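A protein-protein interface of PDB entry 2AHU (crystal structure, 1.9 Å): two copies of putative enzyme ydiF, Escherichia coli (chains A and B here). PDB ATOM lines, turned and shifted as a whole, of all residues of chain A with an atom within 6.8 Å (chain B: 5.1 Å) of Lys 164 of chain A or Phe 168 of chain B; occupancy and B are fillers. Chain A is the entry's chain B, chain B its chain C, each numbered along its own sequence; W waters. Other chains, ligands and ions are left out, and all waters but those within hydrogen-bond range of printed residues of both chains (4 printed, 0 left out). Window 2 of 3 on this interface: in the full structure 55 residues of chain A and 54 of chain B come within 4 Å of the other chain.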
ATOM      1  N   PRO A 133      18.730 -13.304   8.797  1.00  0.00           N
ATOM      2  CA  PRO A 133      18.459 -11.907   9.195  1.00  0.00           C
ATOM      3  C   PRO A 133      19.625 -10.952   8.913  1.00  0.00           C
ATOM      4  O   PRO A 133      19.434  -9.736   8.823  1.00  0.00           O
ATOM      5  CB  PRO A 133      18.191 -12.009  10.699  1.00  0.00           C
ATOM      6  CG  PRO A 133      18.944 -13.237  11.139  1.00  0.00           C
ATOM      7  CD  PRO A 133      18.939 -14.191   9.958  1.00  0.00           C
ATOM      8  N   GLY A 134      20.822 -11.503   8.779  1.00  0.00           N
ATOM      9  CA  GLY A 134      22.000 -10.702   8.492  1.00  0.00           C
ATOM     10  C   GLY A 134      23.244 -11.563   8.496  1.00  0.00           C
ATOM     11  O   GLY A 134      23.165 -12.796   8.676  1.00  0.00           O
ATOM     12  N   ILE A 136      27.501 -11.948   9.845  1.00  0.00           N
ATOM     13  CA  ILE A 136      28.519 -11.594  10.838  1.00  0.00           C
ATOM     14  C   ILE A 136      29.876 -11.570  10.160  1.00  0.00           C
ATOM     15  O   ILE A 136      30.315 -12.575   9.597  1.00  0.00           O
ATOM     16  CB  ILE A 136      28.526 -12.604  12.003  1.00  0.00           C
ATOM     17  CG1 ILE A 136      27.118 -12.770  12.579  1.00  0.00           C
ATOM     18  CG2 ILE A 136      29.469 -12.154  13.112  1.00  0.00           C
ATOM     19  CD1 ILE A 136      26.963 -14.043  13.389  1.00  0.00           C
ATOM     20  N   VAL A 145      32.186   2.398   8.739  1.00  0.00           N
ATOM     21  CA  VAL A 145      31.080   1.432   8.750  1.00  0.00           C
ATOM     22  C   VAL A 145      30.803   0.865  10.165  1.00  0.00           C
ATOM     23  O   VAL A 145      29.676   0.467  10.480  1.00  0.00           O
ATOM     24  CB  VAL A 145      31.334   0.309   7.705  1.00  0.00           C
ATOM     25  CG1 VAL A 145      30.304  -0.783   7.815  1.00  0.00           C
ATOM     26  CG2 VAL A 145      31.317   0.896   6.291  1.00  0.00           C
ATOM     27  N   PRO A 147      29.821   0.918  13.874  1.00  0.00           N
ATOM     28  CA  PRO A 147      28.881   1.786  14.591  1.00  0.00           C
ATOM     29  C   PRO A 147      29.531   2.659  15.671  1.00  0.00           C
ATOM     30  O   PRO A 147      28.920   3.624  16.114  1.00  0.00           O
ATOM     31  CB  PRO A 147      27.877   0.796  15.200  1.00  0.00           C
ATOM     32  CG  PRO A 147      28.591  -0.485  15.252  1.00  0.00           C
ATOM     33  CD  PRO A 147      29.498  -0.508  14.060  1.00  0.00           C
ATOM     34  N   ASP A 161      20.031   2.465  12.863  1.00  0.00           N
ATOM     35  CA  ASP A 161      21.189   1.574  12.838  1.00  0.00           C
ATOM     36  C   ASP A 161      20.869   0.319  12.019  1.00  0.00           C
ATOM     37  O   ASP A 161      19.836  -0.324  12.233  1.00  0.00           O
ATOM     38  CB  ASP A 161      21.589   1.137  14.256  1.00  0.00           C
ATOM     39  CG  ASP A 161      21.849   2.312  15.209  1.00  0.00           C
ATOM     40  OD1 ASP A 161      22.247   3.407  14.760  1.00  0.00           O
ATOM     41  OD2 ASP A 161      21.701   2.214  16.447  1.00  0.00           O
ATOM     42  N   LEU A 162      21.751  -0.020  11.083  1.00  0.00           N
ATOM     43  CA  LEU A 162      21.659  -1.279  10.342  1.00  0.00           C
ATOM     44  C   LEU A 162      22.803  -2.217  10.707  1.00  0.00           C
ATOM     45  O   LEU A 162      22.766  -3.408  10.382  1.00  0.00           O
ATOM     46  CB  LEU A 162      21.694  -1.016   8.834  1.00  0.00           C
ATOM     47  CG  LEU A 162      20.498  -0.309   8.198  1.00  0.00           C
ATOM     48  CD1 LEU A 162      20.781  -0.095   6.725  1.00  0.00           C
ATOM     49  CD2 LEU A 162      19.225  -1.120   8.375  1.00  0.00           C
ATOM     50  N   ILE A 163      23.819  -1.666  11.367  1.00  0.00           N
ATOM     51  CA  ILE A 163      25.020  -2.413  11.728  1.00  0.00           C
ATOM     52  C   ILE A 163      25.218  -2.354  13.239  1.00  0.00           C
ATOM     53  O   ILE A 163      25.046  -1.295  13.849  1.00  0.00           O
ATOM     54  CB  ILE A 163      26.267  -1.850  10.985  1.00  0.00           C
ATOM     55  CG1 ILE A 163      25.989  -1.762   9.471  1.00  0.00           C
ATOM     56  CG2 ILE A 163      27.507  -2.714  11.284  1.00  0.00           C
ATOM     57  CD1 ILE A 163      26.992  -0.950   8.670  1.00  0.00           C
ATOM     58  N   LYS A 164      25.562  -3.486  13.843  1.00  0.00           N
ATOM     59  CA  LYS A 164      25.888  -3.492  15.272  1.00  0.00           C
ATOM     60  C   LYS A 164      27.128  -4.323  15.600  1.00  0.00           C
ATOM     61  O   LYS A 164      27.486  -5.241  14.866  1.00  0.00           O
ATOM     62  CB  LYS A 164      24.684  -3.909  16.120  1.00  0.00           C
ATOM     63  CG  LYS A 164      24.371  -5.384  16.134  1.00  0.00           C
ATOM     64  CD  LYS A 164      23.325  -5.705  17.217  1.00  0.00           C
ATOM     65  CE  LYS A 164      22.908  -7.174  17.135  1.00  0.00           C
ATOM     66  NZ  LYS A 164      21.603  -7.445  17.836  1.00  0.00           N
ATOM     67  N   LEU A 165      27.788  -3.971  16.698  1.00  0.00           N
ATOM     68  CA  LEU A 165      28.971  -4.687  17.147  1.00  0.00           C
ATOM     69  C   LEU A 165      28.519  -5.916  17.916  1.00  0.00           C
ATOM     70  O   LEU A 165      27.629  -5.829  18.758  1.00  0.00           O
ATOM     71  CB  LEU A 165      29.832  -3.778  18.040  1.00  0.00           C
ATOM     72  CG  LEU A 165      31.302  -4.111  18.359  1.00  0.00           C
ATOM     73  CD1 LEU A 165      31.466  -5.342  19.239  1.00  0.00           C
ATOM     74  CD2 LEU A 165      32.138  -4.244  17.096  1.00  0.00           C
ATOM     75  N   VAL A 166      29.120  -7.062  17.601  1.00  0.00           N
ATOM     76  CA  VAL A 166      28.820  -8.311  18.293  1.00  0.00           C
ATOM     77  C   VAL A 166      30.137  -9.004  18.649  1.00  0.00           C
ATOM     78  O   VAL A 166      31.204  -8.597  18.177  1.00  0.00           O
ATOM     79  CB  VAL A 166      27.911  -9.253  17.448  1.00  0.00           C
ATOM     80  CG1 VAL A 166      26.545  -8.616  17.200  1.00  0.00           C
ATOM     81  CG2 VAL A 166      28.586  -9.642  16.130  1.00  0.00           C
ATOM     82  N   PHE A 168      31.985 -12.941  19.028  1.00  0.00           N
ATOM     83  CA  PHE A 168      32.033 -14.396  18.908  1.00  0.00           C
ATOM     84  C   PHE A 168      33.465 -14.866  19.107  1.00  0.00           C
ATOM     85  O   PHE A 168      34.394 -14.266  18.573  1.00  0.00           O
ATOM     86  CB  PHE A 168      31.486 -14.851  17.549  1.00  0.00           C
ATOM     87  CG  PHE A 168      30.005 -14.645  17.398  1.00  0.00           C
ATOM     88  CD1 PHE A 168      29.110 -15.625  17.817  1.00  0.00           C
ATOM     89  CD2 PHE A 168      29.503 -13.466  16.857  1.00  0.00           C
ATOM     90  CE1 PHE A 168      27.738 -15.437  17.691  1.00  0.00           C
ATOM     91  CE2 PHE A 168      28.129 -13.267  16.724  1.00  0.00           C
ATOM     92  CZ  PHE A 168      27.244 -14.253  17.142  1.00  0.00           C
ATOM     93  N   TYR A 173      33.147  -8.510  15.906  1.00  0.00           N
ATOM     94  CA  TYR A 173      32.620  -8.613  14.548  1.00  0.00           C
ATOM     95  C   TYR A 173      31.520  -7.587  14.375  1.00  0.00           C
ATOM     96  O   TYR A 173      30.998  -7.066  15.357  1.00  0.00           O
ATOM     97  CB  TYR A 173      32.048 -10.006  14.277  1.00  0.00           C
ATOM     98  CG  TYR A 173      33.052 -11.140  14.305  1.00  0.00           C
ATOM     99  CD1 TYR A 173      33.776 -11.488  13.166  1.00  0.00           C
ATOM    100  CD2 TYR A 173      33.261 -11.874  15.468  1.00  0.00           C
ATOM    101  CE1 TYR A 173      34.697 -12.539  13.193  1.00  0.00           C
ATOM    102  CE2 TYR A 173      34.176 -12.913  15.505  1.00  0.00           C
ATOM    103  CZ  TYR A 173      34.890 -13.238  14.371  1.00  0.00           C
ATOM    104  OH  TYR A 173      35.785 -14.287  14.409  1.00  0.00           O
ATOM    105  N   LEU A 174      31.176  -7.304  13.118  1.00  0.00           N
ATOM    106  CA  LEU A 174      30.019  -6.490  12.788  1.00  0.00           C
ATOM    107  C   LEU A 174      28.882  -7.397  12.325  1.00  0.00           C
ATOM    108  O   LEU A 174      29.102  -8.320  11.537  1.00  0.00           O
ATOM    109  CB  LEU A 174      30.369  -5.469  11.691  1.00  0.00           C
ATOM    110  CG  LEU A 174      31.426  -4.427  12.081  1.00  0.00           C
ATOM    111  CD1 LEU A 174      31.641  -3.408  10.961  1.00  0.00           C
ATOM    112  CD2 LEU A 174      31.022  -3.713  13.392  1.00  0.00           C
ATOM    113  N   TYR A 175      27.681  -7.145  12.834  1.00  0.00           N
ATOM    114  CA  TYR A 175      26.478  -7.778  12.307  1.00  0.00           C
ATOM    115  C   TYR A 175      25.800  -6.793  11.372  1.00  0.00           C
ATOM    116  O   TYR A 175      25.407  -5.697  11.791  1.00  0.00           O
ATOM    117  CB  TYR A 175      25.529  -8.181  13.440  1.00  0.00           C
ATOM    118  CG  TYR A 175      24.152  -8.584  12.974  1.00  0.00           C
ATOM    119  CD1 TYR A 175      23.899  -9.874  12.521  1.00  0.00           C
ATOM    120  CD2 TYR A 175      23.103  -7.669  12.983  1.00  0.00           C
ATOM    121  CE1 TYR A 175      22.629 -10.248  12.085  1.00  0.00           C
ATOM    122  CE2 TYR A 175      21.828  -8.030  12.543  1.00  0.00           C
ATOM    123  CZ  TYR A 175      21.602  -9.322  12.104  1.00  0.00           C
ATOM    124  OH  TYR A 175      20.343  -9.682  11.683  1.00  0.00           O
ATOM    125  N   TYR A 176      25.664  -7.186  10.108  1.00  0.00           N
ATOM    126  CA  TYR A 176      25.025  -6.354   9.100  1.00  0.00           C
ATOM    127  C   TYR A 176      23.630  -6.912   8.828  1.00  0.00           C
ATOM    128  O   TYR A 176      23.494  -8.067   8.431  1.00  0.00           O
ATOM    129  CB  TYR A 176      25.814  -6.397   7.782  1.00  0.00           C
ATOM    130  CG  TYR A 176      27.193  -5.739   7.746  1.00  0.00           C
ATOM    131  CD1 TYR A 176      27.362  -4.463   7.208  1.00  0.00           C
ATOM    132  CD2 TYR A 176      28.328  -6.422   8.190  1.00  0.00           C
ATOM    133  CE1 TYR A 176      28.631  -3.868   7.129  1.00  0.00           C
ATOM    134  CE2 TYR A 176      29.599  -5.833   8.127  1.00  0.00           C
ATOM    135  CZ  TYR A 176      29.741  -4.559   7.591  1.00  0.00           C
ATOM    136  OH  TYR A 176      30.996  -3.987   7.503  1.00  0.00           O
ATOM    137  N   LYS A 177      22.608  -6.084   9.020  1.00  0.00           N
ATOM    138  CA  LYS A 177      21.228  -6.447   8.699  1.00  0.00           C
ATOM    139  C   LYS A 177      21.056  -6.763   7.206  1.00  0.00           C
ATOM    140  O   LYS A 177      21.515  -6.003   6.344  1.00  0.00           O
ATOM    141  CB  LYS A 177      20.270  -5.322   9.104  1.00  0.00           C
ATOM    142  CG  LYS A 177      18.789  -5.688   8.992  1.00  0.00           C
ATOM    143  CD  LYS A 177      17.914  -4.733   9.788  1.00  0.00           C
ATOM    144  CE  LYS A 177      16.428  -4.959   9.480  1.00  0.00           C
ATOM    145  NZ  LYS A 177      15.910  -6.271   9.986  1.00  0.00           N
ATOM    146  N   ILE B 136      23.734 -17.485  10.789  1.00  0.00           N
ATOM    147  CA  ILE B 136      22.468 -17.360  11.509  1.00  0.00           C
ATOM    148  C   ILE B 136      21.339 -17.866  10.634  1.00  0.00           C
ATOM    149  O   ILE B 136      21.093 -17.319   9.545  1.00  0.00           O
ATOM    150  CB  ILE B 136      22.189 -15.887  11.884  1.00  0.00           C
ATOM    151  CG1 ILE B 136      23.374 -15.272  12.626  1.00  0.00           C
ATOM    152  CG2 ILE B 136      20.928 -15.787  12.743  1.00  0.00           C
ATOM    153  CD1 ILE B 136      23.338 -13.753  12.633  1.00  0.00           C
ATOM    154  N   VAL B 166      20.130 -17.792  19.144  1.00  0.00           N
ATOM    155  CA  VAL B 166      20.274 -16.335  19.094  1.00  0.00           C
ATOM    156  C   VAL B 166      18.930 -15.697  18.723  1.00  0.00           C
ATOM    157  O   VAL B 166      17.997 -16.400  18.326  1.00  0.00           O
ATOM    158  CB  VAL B 166      21.401 -15.881  18.123  1.00  0.00           C
ATOM    159  CG1 VAL B 166      22.752 -16.433  18.554  1.00  0.00           C
ATOM    160  CG2 VAL B 166      21.091 -16.281  16.675  1.00  0.00           C
ATOM    161  N   GLU B 167      18.825 -14.374  18.858  1.00  0.00           N
ATOM    162  CA  GLU B 167      17.580 -13.673  18.541  1.00  0.00           C
ATOM    163  C   GLU B 167      17.813 -12.399  17.744  1.00  0.00           C
ATOM    164  O   GLU B 167      18.688 -11.612  18.094  1.00  0.00           O
ATOM    165  CB  GLU B 167      16.839 -13.330  19.836  1.00  0.00           C
ATOM    166  CG  GLU B 167      15.976 -14.460  20.376  1.00  0.00           C
ATOM    167  CD  GLU B 167      14.495 -14.203  20.178  1.00  0.00           C
ATOM    168  OE1 GLU B 167      13.685 -15.023  20.668  1.00  0.00           O
ATOM    169  OE2 GLU B 167      14.127 -13.174  19.550  1.00  0.00           O
ATOM    170  N   PHE B 168      17.032 -12.214  16.679  1.00  0.00           N
ATOM    171  CA  PHE B 168      17.076 -11.004  15.843  1.00  0.00           C
ATOM    172  C   PHE B 168      15.667 -10.671  15.379  1.00  0.00           C
ATOM    173  O   PHE B 168      14.907 -11.580  15.031  1.00  0.00           O
ATOM    174  CB  PHE B 168      17.990 -11.193  14.622  1.00  0.00           C
ATOM    175  CG  PHE B 168      19.434 -11.345  14.971  1.00  0.00           C
ATOM    176  CD1 PHE B 168      20.240 -10.225  15.125  1.00  0.00           C
ATOM    177  CD2 PHE B 168      19.993 -12.605  15.174  1.00  0.00           C
ATOM    178  CE1 PHE B 168      21.578 -10.358  15.466  1.00  0.00           C
ATOM    179  CE2 PHE B 168      21.332 -12.742  15.514  1.00  0.00           C
ATOM    180  CZ  PHE B 168      22.124 -11.611  15.660  1.00  0.00           C
ATOM    181  N   ASP B 169      15.317  -9.381  15.401  1.00  0.00           N
ATOM    182  CA  ASP B 169      14.020  -8.889  14.905  1.00  0.00           C
ATOM    183  C   ASP B 169      12.830  -9.595  15.557  1.00  0.00           C
ATOM    184  O   ASP B 169      11.831  -9.890  14.884  1.00  0.00           O
ATOM    185  CB  ASP B 169      13.917  -9.067  13.380  1.00  0.00           C
ATOM    186  CG  ASP B 169      15.054  -8.421  12.638  1.00  0.00           C
ATOM    187  OD1 ASP B 169      15.213  -7.187  12.781  1.00  0.00           O
ATOM    188  OD2 ASP B 169      15.821  -9.065  11.880  1.00  0.00           O
ATOM    189  N   ASN B 170      12.958  -9.880  16.850  1.00  0.00           N
ATOM    190  CA  ASN B 170      11.926 -10.597  17.623  1.00  0.00           C
ATOM    191  C   ASN B 170      11.611 -12.028  17.123  1.00  0.00           C
ATOM    192  O   ASN B 170      10.482 -12.521  17.263  1.00  0.00           O
ATOM    193  CB  ASN B 170      10.650  -9.737  17.775  1.00  0.00           C
ATOM    194  CG  ASN B 170       9.831 -10.114  19.005  1.00  0.00           C
ATOM    195  OD1 ASN B 170       8.597 -10.055  18.993  1.00  0.00           O
ATOM    196  ND2 ASN B 170      10.514 -10.504  20.066  1.00  0.00           N
ATOM    197  N   LYS B 171      12.627 -12.692  16.561  1.00  0.00           N
ATOM    198  CA  LYS B 171      12.521 -14.072  16.077  1.00  0.00           C
ATOM    199  C   LYS B 171      13.718 -14.913  16.546  1.00  0.00           C
ATOM    200  O   LYS B 171      14.839 -14.400  16.690  1.00  0.00           O
ATOM    201  CB  LYS B 171      12.434 -14.100  14.540  1.00  0.00           C
ATOM    202  CG  LYS B 171      11.170 -13.460  13.964  1.00  0.00           C
ATOM    203  CD  LYS B 171      11.297 -13.224  12.452  1.00  0.00           C
ATOM    204  CE  LYS B 171      11.431 -14.538  11.684  1.00  0.00           C
ATOM    205  NZ  LYS B 171      10.109 -15.129  11.322  1.00  0.00           N
ATOM    206  N   TYR B 173      16.620 -17.717  16.148  1.00  0.00           N
ATOM    207  CA  TYR B 173      17.481 -18.312  15.132  1.00  0.00           C
ATOM    208  C   TYR B 173      18.506 -19.196  15.806  1.00  0.00           C
ATOM    209  O   TYR B 173      18.757 -19.058  17.008  1.00  0.00           O
ATOM    210  CB  TYR B 173      18.217 -17.225  14.351  1.00  0.00           C
ATOM    211  CG  TYR B 173      17.311 -16.347  13.533  1.00  0.00           C
ATOM    212  CD1 TYR B 173      16.910 -16.729  12.252  1.00  0.00           C
ATOM    213  CD2 TYR B 173      16.835 -15.135  14.045  1.00  0.00           C
ATOM    214  CE1 TYR B 173      16.056 -15.916  11.493  1.00  0.00           C
ATOM    215  CE2 TYR B 173      15.991 -14.320  13.296  1.00  0.00           C
ATOM    216  CZ  TYR B 173      15.605 -14.712  12.031  1.00  0.00           C
ATOM    217  OH  TYR B 173      14.766 -13.904  11.296  1.00  0.00           O
HETATM  218  O   HOH W   1      17.013  -8.655   8.619  1.00  0.00           O
HETATM  219  O   HOH W   2      24.304 -15.438   8.699  1.00  0.00           O
HETATM  220  O   HOH W   3      19.238  -9.027  18.381  1.00  0.00           O
HETATM  221  O   HOH W   4      18.451  -7.972  12.185  1.00  0.00           O
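Ile 136 of chain B touches its own counterpart, Ile 136 of chain A. 4 positions are printed for both chains. Of the 8 pairs that touch across the chains among the printed residues, 1 has its exchanged pair printed and touching as well.
Of the printed residues of chain B, Pro 133 of chain A touches Ile 136, Asp 169 and Tyr 173. Of the printed residues of chain B, Ile 136 of chain A touches Ile 136 (3.7 Å). Lys 164 of chain A touches one residue of chain B. Of the printed residues of chain B, Tyr 175 of chain A touches Ile 136 and Phe 168. Of the printed residues of chain A, Phe 168 of chain B touches Lys 164 and Tyr 175. The nearest printed residue of chain A that does not touch Asp 169 of chain B is Tyr 175 of chain A (4.6 Å).
Of the 8 printed residues of chain B, 4 touch a printed residue of chain A. Among the printed residues, 8 pairs touch across the chains. Among the printed residues, Asp or Glu carboxylates within 4 Å of a Lys or Arg side-chain nitrogen of the other chain: Lys 177 of chain A with Asp 169 of chain B (3.0 Å).
Among the printed residues, pairs that only touch across the chains: Tyr 175 of chain A with Phe 168 of chain B, Pro 133 of chain A with Ile 136 of chain B, Tyr 175 of chain A with Ile 136 of chain B, Pro 133 of chain A with Tyr 173 of chain B, Ile 136 of chain A with Ile 136 of chain B, Lys 164 of chain A with Phe 168 of chain B and Pro 133 of chain A with Asp 169 of chain B.
The backbone carbonyl oxygen (O) of Pro 133 of chain A is in hydrogen-bond range of the side-chain hydroxyl (OH) of Tyr 175 of chain A (3.0 Å). The side-chain hydroxyl (OH) of Tyr 175 of chain A lies within hydrogen-bond range of the backbone NH (N) of Gly 134 of chain A. N of Lys 177 of chain A sits at hydrogen-bond distance from O of Leu 162 of chain A, 3.0 Å away. The backbone carbonyl oxygen (O) of Lys 164 of chain A is in hydrogen-bond range of the backbone NH (N) of Tyr 175 of chain A, at 2.8 Å. The backbone carbonyl oxygen of Tyr 173 of chain B is in hydrogen-bond range of the backbone NH of Val 166 of chain B (2.8 Å).
NZ of Lys 177 of chain A is in salt-bridge range of OD1 of Asp 169 of chain B.
Water W4 lies within hydrogen-bond range of the side-chain hydroxyl (OH) of Tyr 175 of chain A (2.6 Å) and the side-chain carboxylate (OD2) of Asp 169 of chain B (2.9 Å). Water W3 bridges the backbone carbonyl oxygen of Glu 167 of chain B (2.7 Å) and the side-chain amino group of Lys 164 of chain A (2.9 Å). Water W1 lies within hydrogen-bond range of the backbone carbonyl oxygen of Pro 133 of chain A, the side-chain amino group of Lys 177 of chain A and the side-chain carboxylate of Asp 169 of chain B. Water W2 lies within hydrogen-bond range of O of Gly 134 of chain A (2.9 Å) and N of Ile 136 of chain B (3.0 Å).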
